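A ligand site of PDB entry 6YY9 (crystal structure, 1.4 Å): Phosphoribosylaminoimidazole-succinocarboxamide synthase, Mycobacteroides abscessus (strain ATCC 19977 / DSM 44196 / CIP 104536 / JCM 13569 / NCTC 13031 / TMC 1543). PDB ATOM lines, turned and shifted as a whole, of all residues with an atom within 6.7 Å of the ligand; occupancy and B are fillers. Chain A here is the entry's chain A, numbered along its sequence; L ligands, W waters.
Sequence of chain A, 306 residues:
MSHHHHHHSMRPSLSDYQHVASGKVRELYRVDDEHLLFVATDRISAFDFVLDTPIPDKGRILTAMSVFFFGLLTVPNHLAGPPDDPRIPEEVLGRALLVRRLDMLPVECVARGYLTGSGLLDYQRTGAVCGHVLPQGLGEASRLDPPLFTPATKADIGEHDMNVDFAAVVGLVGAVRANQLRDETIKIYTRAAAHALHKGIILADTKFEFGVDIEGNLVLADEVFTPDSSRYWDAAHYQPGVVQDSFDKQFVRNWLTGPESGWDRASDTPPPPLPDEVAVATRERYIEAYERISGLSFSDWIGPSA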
ATOM      1  N   VAL A  20     -25.898   5.144  13.882  1.00  0.00           N
ATOM      2  CA  VAL A  20     -26.266   6.533  13.613  1.00  0.00           C
ATOM      3  C   VAL A  20     -25.076   7.456  13.416  1.00  0.00           C
ATOM      4  O   VAL A  20     -25.214   8.538  12.859  1.00  0.00           O
ATOM      5  CB  VAL A  20     -27.128   7.126  14.749  1.00  0.00           C
ATOM      6  CG1 VAL A  20     -28.459   6.409  14.823  1.00  0.00           C
ATOM      7  CG2 VAL A  20     -26.388   7.068  16.085  1.00  0.00           C
ATOM      8  N   ALA A  21     -23.903   7.047  13.882  1.00  0.00           N
ATOM      9  CA  ALA A  21     -22.751   7.932  13.773  1.00  0.00           C
ATOM     10  C   ALA A  21     -21.479   7.169  14.009  1.00  0.00           C
ATOM     11  O   ALA A  21     -21.425   6.212  14.783  1.00  0.00           O
ATOM     12  CB  ALA A  21     -22.872   9.115  14.755  1.00  0.00           C
ATOM     13  N   SER A  22     -20.444   7.595  13.308  1.00  0.00           N
ATOM     14  CA  SER A  22     -19.118   7.050  13.501  1.00  0.00           C
ATOM     15  C   SER A  22     -18.128   8.191  13.525  1.00  0.00           C
ATOM     16  O   SER A  22     -18.305   9.202  12.833  1.00  0.00           O
ATOM     17  CB  SER A  22     -18.759   6.053  12.399  1.00  0.00           C
ATOM     18  OG  SER A  22     -19.451   4.832  12.575  1.00  0.00           O
ATOM     19  N   GLY A  23     -17.120   8.043  14.361  1.00  0.00           N
ATOM     20  CA  GLY A  23     -15.956   8.893  14.301  1.00  0.00           C
ATOM     21  C   GLY A  23     -14.793   8.011  13.894  1.00  0.00           C
ATOM     22  O   GLY A  23     -14.994   6.900  13.400  1.00  0.00           O
ATOM     23  N   LYS A  24     -13.577   8.497  14.118  1.00  0.00           N
ATOM     24  CA  LYS A  24     -12.389   7.751  13.740  1.00  0.00           C
ATOM     25  C   LYS A  24     -12.350   6.395  14.446  1.00  0.00           C
ATOM     26  O   LYS A  24     -12.127   5.365  13.808  1.00  0.00           O
ATOM     27  CB  LYS A  24     -11.136   8.554  14.066  1.00  0.00           C
ATOM     28  N   VAL A  25     -12.574   6.404  15.760  1.00  0.00           N
ATOM     29  CA  VAL A  25     -12.393   5.206  16.560  1.00  0.00           C
ATOM     30  C   VAL A  25     -13.567   4.884  17.479  1.00  0.00           C
ATOM     31  O   VAL A  25     -13.482   3.975  18.289  1.00  0.00           O
ATOM     32  CB  VAL A  25     -11.109   5.310  17.425  1.00  0.00           C
ATOM     33  CG1 VAL A  25      -9.913   5.740  16.584  1.00  0.00           C
ATOM     34  CG2 VAL A  25     -11.311   6.270  18.575  1.00  0.00           C
ATOM     35  N   ARG A  26     -14.661   5.630  17.369  1.00  0.00           N
ATOM     36  CA  ARG A  26     -15.860   5.313  18.128  1.00  0.00           C
ATOM     37  C   ARG A  26     -17.077   5.181  17.231  1.00  0.00           C
ATOM     38  O   ARG A  26     -17.097   5.697  16.122  1.00  0.00           O
ATOM     39  CB  ARG A  26     -16.121   6.377  19.189  1.00  0.00           C
ATOM     40  CG  ARG A  26     -14.964   6.596  20.111  1.00  0.00           C
ATOM     41  CD  ARG A  26     -15.249   7.790  20.928  1.00  0.00           C
ATOM     42  NE  ARG A  26     -15.479   8.965  20.099  1.00  0.00           N
ATOM     43  CZ  ARG A  26     -15.749  10.157  20.608  1.00  0.00           C
ATOM     44  NH1 ARG A  26     -15.810  10.297  21.920  1.00  0.00           N
ATOM     45  NH2 ARG A  26     -15.957  11.195  19.817  1.00  0.00           N
ATOM     46  N   GLU A  27     -18.094   4.499  17.744  1.00  0.00           N
ATOM     47  CA  GLU A  27     -19.322   4.282  16.997  1.00  0.00           C
ATOM     48  C   GLU A  27     -20.508   4.544  17.896  1.00  0.00           C
ATOM     49  O   GLU A  27     -20.406   4.372  19.114  1.00  0.00           O
ATOM     50  CB  GLU A  27     -19.383   2.843  16.476  1.00  0.00           C
ATOM     51  CG  GLU A  27     -18.308   2.477  15.467  1.00  0.00           C
ATOM     52  CD  GLU A  27     -18.300   0.997  15.144  1.00  0.00           C
ATOM     53  OE1 GLU A  27     -18.791   0.192  15.965  1.00  0.00           O
ATOM     54  OE2 GLU A  27     -17.792   0.627  14.056  1.00  0.00           O
ATOM     55  N   LEU A  28     -21.616   4.945  17.299  1.00  0.00           N
ATOM     56  CA  LEU A  28     -22.825   5.229  18.053  1.00  0.00           C
ATOM     57  C   LEU A  28     -24.028   4.527  17.422  1.00  0.00           C
ATOM     58  O   LEU A  28     -24.187   4.564  16.187  1.00  0.00           O
ATOM     59  CB  LEU A  28     -23.041   6.745  18.110  1.00  0.00           C
ATOM     60  CG  LEU A  28     -24.035   7.301  19.113  1.00  0.00           C
ATOM     61  CD1 LEU A  28     -23.643   6.946  20.546  1.00  0.00           C
ATOM     62  CD2 LEU A  28     -24.098   8.816  18.944  1.00  0.00           C
ATOM     63  N   LEU A  36     -28.943   5.388  23.523  1.00  0.00           N
ATOM     64  CA  LEU A  36     -27.940   5.043  22.536  1.00  0.00           C
ATOM     65  C   LEU A  36     -26.954   4.059  23.131  1.00  0.00           C
ATOM     66  O   LEU A  36     -26.852   3.887  24.349  1.00  0.00           O
ATOM     67  CB  LEU A  36     -27.193   6.283  22.049  1.00  0.00           C
ATOM     68  CG  LEU A  36     -28.051   7.473  21.595  1.00  0.00           C
ATOM     69  CD1 LEU A  36     -27.195   8.700  21.341  1.00  0.00           C
ATOM     70  CD2 LEU A  36     -28.869   7.114  20.366  1.00  0.00           C
ATOM     71  N   PHE A  38     -22.929   3.579  23.053  1.00  0.00           N
ATOM     72  CA  PHE A  38     -21.680   4.268  22.756  1.00  0.00           C
ATOM     73  C   PHE A  38     -20.558   3.239  22.731  1.00  0.00           C
ATOM     74  O   PHE A  38     -20.241   2.655  23.772  1.00  0.00           O
ATOM     75  CB  PHE A  38     -21.452   5.342  23.829  1.00  0.00           C
ATOM     76  CG  PHE A  38     -20.340   6.318  23.521  1.00  0.00           C
ATOM     77  CD1 PHE A  38     -19.020   5.922  23.524  1.00  0.00           C
ATOM     78  CD2 PHE A  38     -20.645   7.658  23.309  1.00  0.00           C
ATOM     79  CE1 PHE A  38     -18.015   6.837  23.267  1.00  0.00           C
ATOM     80  CE2 PHE A  38     -19.641   8.569  23.065  1.00  0.00           C
ATOM     81  CZ  PHE A  38     -18.322   8.160  23.041  1.00  0.00           C
ATOM     82  N   VAL A  39     -19.951   3.023  21.566  1.00  0.00           N
ATOM     83  CA  VAL A  39     -18.983   1.940  21.383  1.00  0.00           C
ATOM     84  C   VAL A  39     -17.570   2.446  21.092  1.00  0.00           C
ATOM     85  O   VAL A  39     -17.368   3.218  20.159  1.00  0.00           O
ATOM     86  CB  VAL A  39     -19.407   1.002  20.232  1.00  0.00           C
ATOM     87  CG1 VAL A  39     -18.388  -0.107  20.031  1.00  0.00           C
ATOM     88  CG2 VAL A  39     -20.801   0.418  20.482  1.00  0.00           C
ATOM     89  N   HIS A  78     -24.260  11.212  30.990  1.00  0.00           N
ATOM     90  CA  HIS A  78     -25.230  10.545  30.140  1.00  0.00           C
ATOM     91  C   HIS A  78     -25.311   9.045  30.335  1.00  0.00           C
ATOM     92  O   HIS A  78     -26.103   8.400  29.656  1.00  0.00           O
ATOM     93  CB  HIS A  78     -24.978  10.909  28.659  1.00  0.00           C
ATOM     94  CG  HIS A  78     -23.779  10.287  28.010  1.00  0.00           C
ATOM     95  ND1 HIS A  78     -22.622   9.889  28.659  1.00  0.00           N
ATOM     96  CD2 HIS A  78     -23.533  10.134  26.692  1.00  0.00           C
ATOM     97  CE1 HIS A  78     -21.749   9.431  27.769  1.00  0.00           C
ATOM     98  NE2 HIS A  78     -22.278   9.585  26.566  1.00  0.00           N
ATOM     99  N   VAL A  99     -26.256   4.808  27.037  1.00  0.00           N
ATOM    100  CA  VAL A  99     -26.356   6.221  27.409  1.00  0.00           C
ATOM    101  C   VAL A  99     -27.715   6.821  27.060  1.00  0.00           C
ATOM    102  O   VAL A  99     -28.446   6.318  26.189  1.00  0.00           O
ATOM    103  CB  VAL A  99     -25.214   7.053  26.745  1.00  0.00           C
ATOM    104  CG1 VAL A  99     -23.858   6.484  27.128  1.00  0.00           C
ATOM    105  CG2 VAL A  99     -25.346   7.098  25.244  1.00  0.00           C
ATOM    106  N   ARG A 100     -28.079   7.882  27.776  1.00  0.00           N
ATOM    107  CA  ARG A 100     -29.311   8.627  27.491  1.00  0.00           C
ATOM    108  C   ARG A 100     -29.130   9.512  26.272  1.00  0.00           C
ATOM    109  O   ARG A 100     -28.118  10.190  26.150  1.00  0.00           O
ATOM    110  CB  ARG A 100     -29.706   9.523  28.681  1.00  0.00           C
ATOM    111  CG  ARG A 100     -29.594   8.989  30.088  1.00  0.00           C
ATOM    112  CD  ARG A 100     -30.125  10.071  31.057  1.00  0.00           C
ATOM    113  NE  ARG A 100     -29.079  10.792  31.792  1.00  0.00           N
ATOM    114  CZ  ARG A 100     -29.225  12.017  32.311  1.00  0.00           C
ATOM    115  NH1 ARG A 100     -30.370  12.675  32.148  1.00  0.00           N
ATOM    116  NH2 ARG A 100     -28.230  12.582  32.968  1.00  0.00           N
ATOM    117  N   ARG A 101     -30.141   9.575  25.399  1.00  0.00           N
ATOM    118  CA  ARG A 101     -30.101  10.513  24.289  1.00  0.00           C
ATOM    119  C   ARG A 101     -30.303  11.953  24.773  1.00  0.00           C
ATOM    120  O   ARG A 101     -31.243  12.240  25.520  1.00  0.00           O
ATOM    121  CB  ARG A 101     -31.161  10.172  23.244  1.00  0.00           C
ATOM    122  CG  ARG A 101     -31.084  11.106  22.038  1.00  0.00           C
ATOM    123  CD  ARG A 101     -31.993  10.688  20.899  1.00  0.00           C
ATOM    124  NE  ARG A 101     -33.399  10.600  21.295  1.00  0.00           N
ATOM    125  CZ  ARG A 101     -34.192  11.647  21.499  1.00  0.00           C
ATOM    126  NH1 ARG A 101     -33.715  12.883  21.343  1.00  0.00           N
ATOM    127  NH2 ARG A 101     -35.453  11.463  21.854  1.00  0.00           N
ATOM    128  N   LEU A 102     -29.398  12.836  24.357  1.00  0.00           N
ATOM    129  CA  LEU A 102     -29.467  14.263  24.708  1.00  0.00           C
ATOM    130  C   LEU A 102     -29.559  15.150  23.475  1.00  0.00           C
ATOM    131  O   LEU A 102     -29.255  14.712  22.370  1.00  0.00           O
ATOM    132  CB  LEU A 102     -28.226  14.666  25.516  1.00  0.00           C
ATOM    133  CG  LEU A 102     -27.923  13.913  26.797  1.00  0.00           C
ATOM    134  CD1 LEU A 102     -26.488  14.192  27.198  1.00  0.00           C
ATOM    135  CD2 LEU A 102     -28.869  14.340  27.895  1.00  0.00           C
ATOM    136  N   ASP A 103     -29.959  16.403  23.659  1.00  0.00           N
ATOM    137  CA  ASP A 103     -29.789  17.407  22.624  1.00  0.00           C
ATOM    138  C   ASP A 103     -28.382  17.977  22.748  1.00  0.00           C
ATOM    139  O   ASP A 103     -28.106  18.743  23.678  1.00  0.00           O
ATOM    140  CB  ASP A 103     -30.844  18.516  22.739  1.00  0.00           C
ATOM    141  CG  ASP A 103     -32.242  18.052  22.367  1.00  0.00           C
ATOM    142  OD1 ASP A 103     -32.361  17.053  21.620  1.00  0.00           O
ATOM    143  OD2 ASP A 103     -33.217  18.687  22.827  1.00  0.00           O
ATOM    144  N   MET A 104     -27.487  17.579  21.851  1.00  0.00           N
ATOM    145  CA  MET A 104     -26.079  17.940  21.990  1.00  0.00           C
ATOM    146  C   MET A 104     -25.836  19.407  21.673  1.00  0.00           C
ATOM    147  O   MET A 104     -26.409  19.945  20.738  1.00  0.00           O
ATOM    148  CB  MET A 104     -25.219  17.054  21.089  1.00  0.00           C
ATOM    149  CG  MET A 104     -25.291  15.578  21.475  1.00  0.00           C
ATOM    150  SD  MET A 104     -24.731  15.225  23.162  1.00  0.00           S
ATOM    151  CE  MET A 104     -23.000  15.657  23.030  1.00  0.00           C
ATOM    152  N   GLU A 209     -17.747  16.992  25.380  1.00  0.00           N
ATOM    153  CA  GLU A 209     -18.996  17.433  24.774  1.00  0.00           C
ATOM    154  C   GLU A 209     -20.120  17.343  25.796  1.00  0.00           C
ATOM    155  O   GLU A 209     -20.165  16.416  26.615  1.00  0.00           O
ATOM    156  CB  GLU A 209     -19.349  16.590  23.544  1.00  0.00           C
ATOM    157  CG  GLU A 209     -18.465  16.899  22.324  1.00  0.00           C
ATOM    158  CD  GLU A 209     -18.827  16.048  21.113  1.00  0.00           C
ATOM    159  OE1 GLU A 209     -19.489  15.003  21.294  1.00  0.00           O
ATOM    160  OE2 GLU A 209     -18.439  16.418  19.989  1.00  0.00           O
ATOM    161  N   LEU A 220     -22.941  15.975  30.984  1.00  0.00           N
ATOM    162  CA  LEU A 220     -21.664  15.601  30.380  1.00  0.00           C
ATOM    163  C   LEU A 220     -21.816  14.315  29.572  1.00  0.00           C
ATOM    164  O   LEU A 220     -22.339  13.313  30.063  1.00  0.00           O
ATOM    165  CB  LEU A 220     -20.604  15.436  31.493  1.00  0.00           C
ATOM    166  CG  LEU A 220     -19.165  15.096  31.114  1.00  0.00           C
ATOM    167  CD1 LEU A 220     -18.554  16.168  30.243  1.00  0.00           C
ATOM    168  CD2 LEU A 220     -18.358  14.915  32.376  1.00  0.00           C
ATOM    169  N   ALA A 221     -21.385  14.350  28.318  1.00  0.00           N
ATOM    170  CA  ALA A 221     -21.597  13.203  27.440  1.00  0.00           C
ATOM    171  C   ALA A 221     -20.267  12.660  26.894  1.00  0.00           C
ATOM    172  O   ALA A 221     -19.214  12.830  27.515  1.00  0.00           O
ATOM    173  CB  ALA A 221     -22.559  13.583  26.324  1.00  0.00           C
ATOM    174  N   ASP A 222     -20.340  11.975  25.751  1.00  0.00           N
ATOM    175  CA  ASP A 222     -19.148  11.478  25.078  1.00  0.00           C
ATOM    176  C   ASP A 222     -18.319  10.595  26.008  1.00  0.00           C
ATOM    177  O   ASP A 222     -18.860   9.823  26.798  1.00  0.00           O
ATOM    178  CB  ASP A 222     -18.324  12.656  24.532  1.00  0.00           C
ATOM    179  CG  ASP A 222     -17.372  12.256  23.421  1.00  0.00           C
ATOM    180  OD1 ASP A 222     -17.829  11.674  22.409  1.00  0.00           O
ATOM    181  OD2 ASP A 222     -16.160  12.510  23.569  1.00  0.00           O
ATOM    182  N   GLU A 223     -16.998  10.702  25.889  1.00  0.00           N
ATOM    183  CA  GLU A 223     -16.088  10.003  26.773  1.00  0.00           C
ATOM    184  C   GLU A 223     -15.302  11.055  27.514  1.00  0.00           C
ATOM    185  O   GLU A 223     -15.119  12.174  27.043  1.00  0.00           O
ATOM    186  CB  GLU A 223     -15.162   9.079  25.994  1.00  0.00           C
ATOM    187  CG  GLU A 223     -14.079   9.785  25.187  1.00  0.00           C
ATOM    188  CD  GLU A 223     -13.434   8.844  24.190  1.00  0.00           C
ATOM    189  OE1 GLU A 223     -12.200   8.924  23.969  1.00  0.00           O
ATOM    190  OE2 GLU A 223     -14.158   8.016  23.619  1.00  0.00           O
HETATM  191  C1  LIG L   1     -23.680  12.123  20.298  1.00  0.00           C
HETATM  192  N1  LIG L   1     -21.732  12.240  19.346  1.00  0.00           N
HETATM  193  C2  LIG L   1     -20.307  12.251  19.128  1.00  0.00           C
HETATM  194  C3  LIG L   1     -19.739  10.446  17.452  1.00  0.00           C
HETATM  195  C4  LIG L   1     -19.487   8.536  19.402  1.00  0.00           C
HETATM  196  C5  LIG L   1     -19.814   9.829  19.767  1.00  0.00           C
HETATM  197  N2  LIG L   1     -25.711  11.004  24.809  1.00  0.00           N
HETATM  198  C6  LIG L   1     -25.832  11.476  23.515  1.00  0.00           C
HETATM  199  N3  LIG L   1     -26.998  11.888  23.044  1.00  0.00           N
HETATM  200  C7  LIG L   1     -27.122  12.332  21.800  1.00  0.00           C
HETATM  201  N4  LIG L   1     -26.070  12.396  20.972  1.00  0.00           N
HETATM  202  C8  LIG L   1     -24.849  12.018  21.341  1.00  0.00           C
HETATM  203  C9  LIG L   1     -24.678  11.528  22.656  1.00  0.00           C
HETATM  204  C10 LIG L   1     -23.325  11.058  23.188  1.00  0.00           C
HETATM  205  N5  LIG L   1     -22.319  10.707  23.603  1.00  0.00           N
HETATM  206  C11 LIG L   1     -22.322  12.130  20.533  1.00  0.00           C
HETATM  207  N6  LIG L   1     -22.651  12.295  18.359  1.00  0.00           N
HETATM  208  C12 LIG L   1     -23.868  12.251  18.935  1.00  0.00           C
HETATM  209  C13 LIG L   1     -19.942  10.820  18.748  1.00  0.00           C
HETATM  210  N7  LIG L   1     -19.428   9.195  17.145  1.00  0.00           N
HETATM  211  C14 LIG L   1     -19.298   8.248  18.067  1.00  0.00           C
HETATM  212  O   HOH W   1     -22.348  12.641  15.519  1.00  0.00           O
HETATM  213  O   HOH W   2     -26.899  13.977  18.690  1.00  0.00           O
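The backbone carbonyl oxygen of Arg 100 lies within hydrogen-bond range of a nitrogen (N2) of the ligand, 2.9 Å away. The backbone NH (N) of Asp 222 sits at hydrogen-bond distance from a nitrogen (N5) of the ligand (3.2 Å). A ring nitrogen (NE2) of His 78 lies within hydrogen-bond range of a nitrogen (N5) of the ligand (3.2 Å). N of Leu 102 sits at hydrogen-bond distance from N3 of the ligand, at 2.9 Å.
N of Glu 27 sits at hydrogen-bond distance from O of Val 39 (2.8 Å). The backbone carbonyl oxygen (O) of Leu 220 sits at hydrogen-bond distance from the backbone NH (N) of His 78, at 3.0 Å. The backbone NH of Leu 36 lies within hydrogen-bond range of the backbone carbonyl oxygen of Val 99. The guanidinium group (NH1) of Arg 26 is in salt-bridge range of the side-chain carboxylate (OD1) of Asp 222 (2.5 Å). O of Leu 28 sits at hydrogen-bond distance from N of Val 20 (2.9 Å). The guanidinium group (NH1) of Arg 26 is in salt-bridge range of the side-chain carboxylate (OE2) of Glu 223 (3.3 Å). The backbone NH of Leu 28 lies within hydrogen-bond range of the backbone carbonyl oxygen of Ala 21, 2.8 Å away. A ring nitrogen (NE2) of His 78 is in hydrogen-bond range of the backbone NH (N) of Asp 222 (3.2 Å).
Ser 22 touches the ligand. Gly 23 touches the ligand (N to N7, 3.8 Å). CB of Arg 26 touches C14 of the ligand, 3.9 Å away. Glu 27 touches the ligand. Leu 28 touches the ligand. Leu 36 touches the ligand (CD1 to N3, 3.6 Å). Phe 38 touches the ligand (CE2 to N5, 3.5 Å). Val 99 touches the ligand (CG2 to N2, 3.9 Å). Arg 101 touches the ligand. Met 104 touches the ligand (CG to N4, 3.3 Å). OE1 of Glu 209 touches C2 of the ligand, at 3.6 Å. Ala 221 touches the ligand. Hydrophobic or aromatic side chains that line the ligand: Leu 28, Leu 36, Phe 38, His 78, Val 99, Leu 102, Met 104 and Ala 221.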
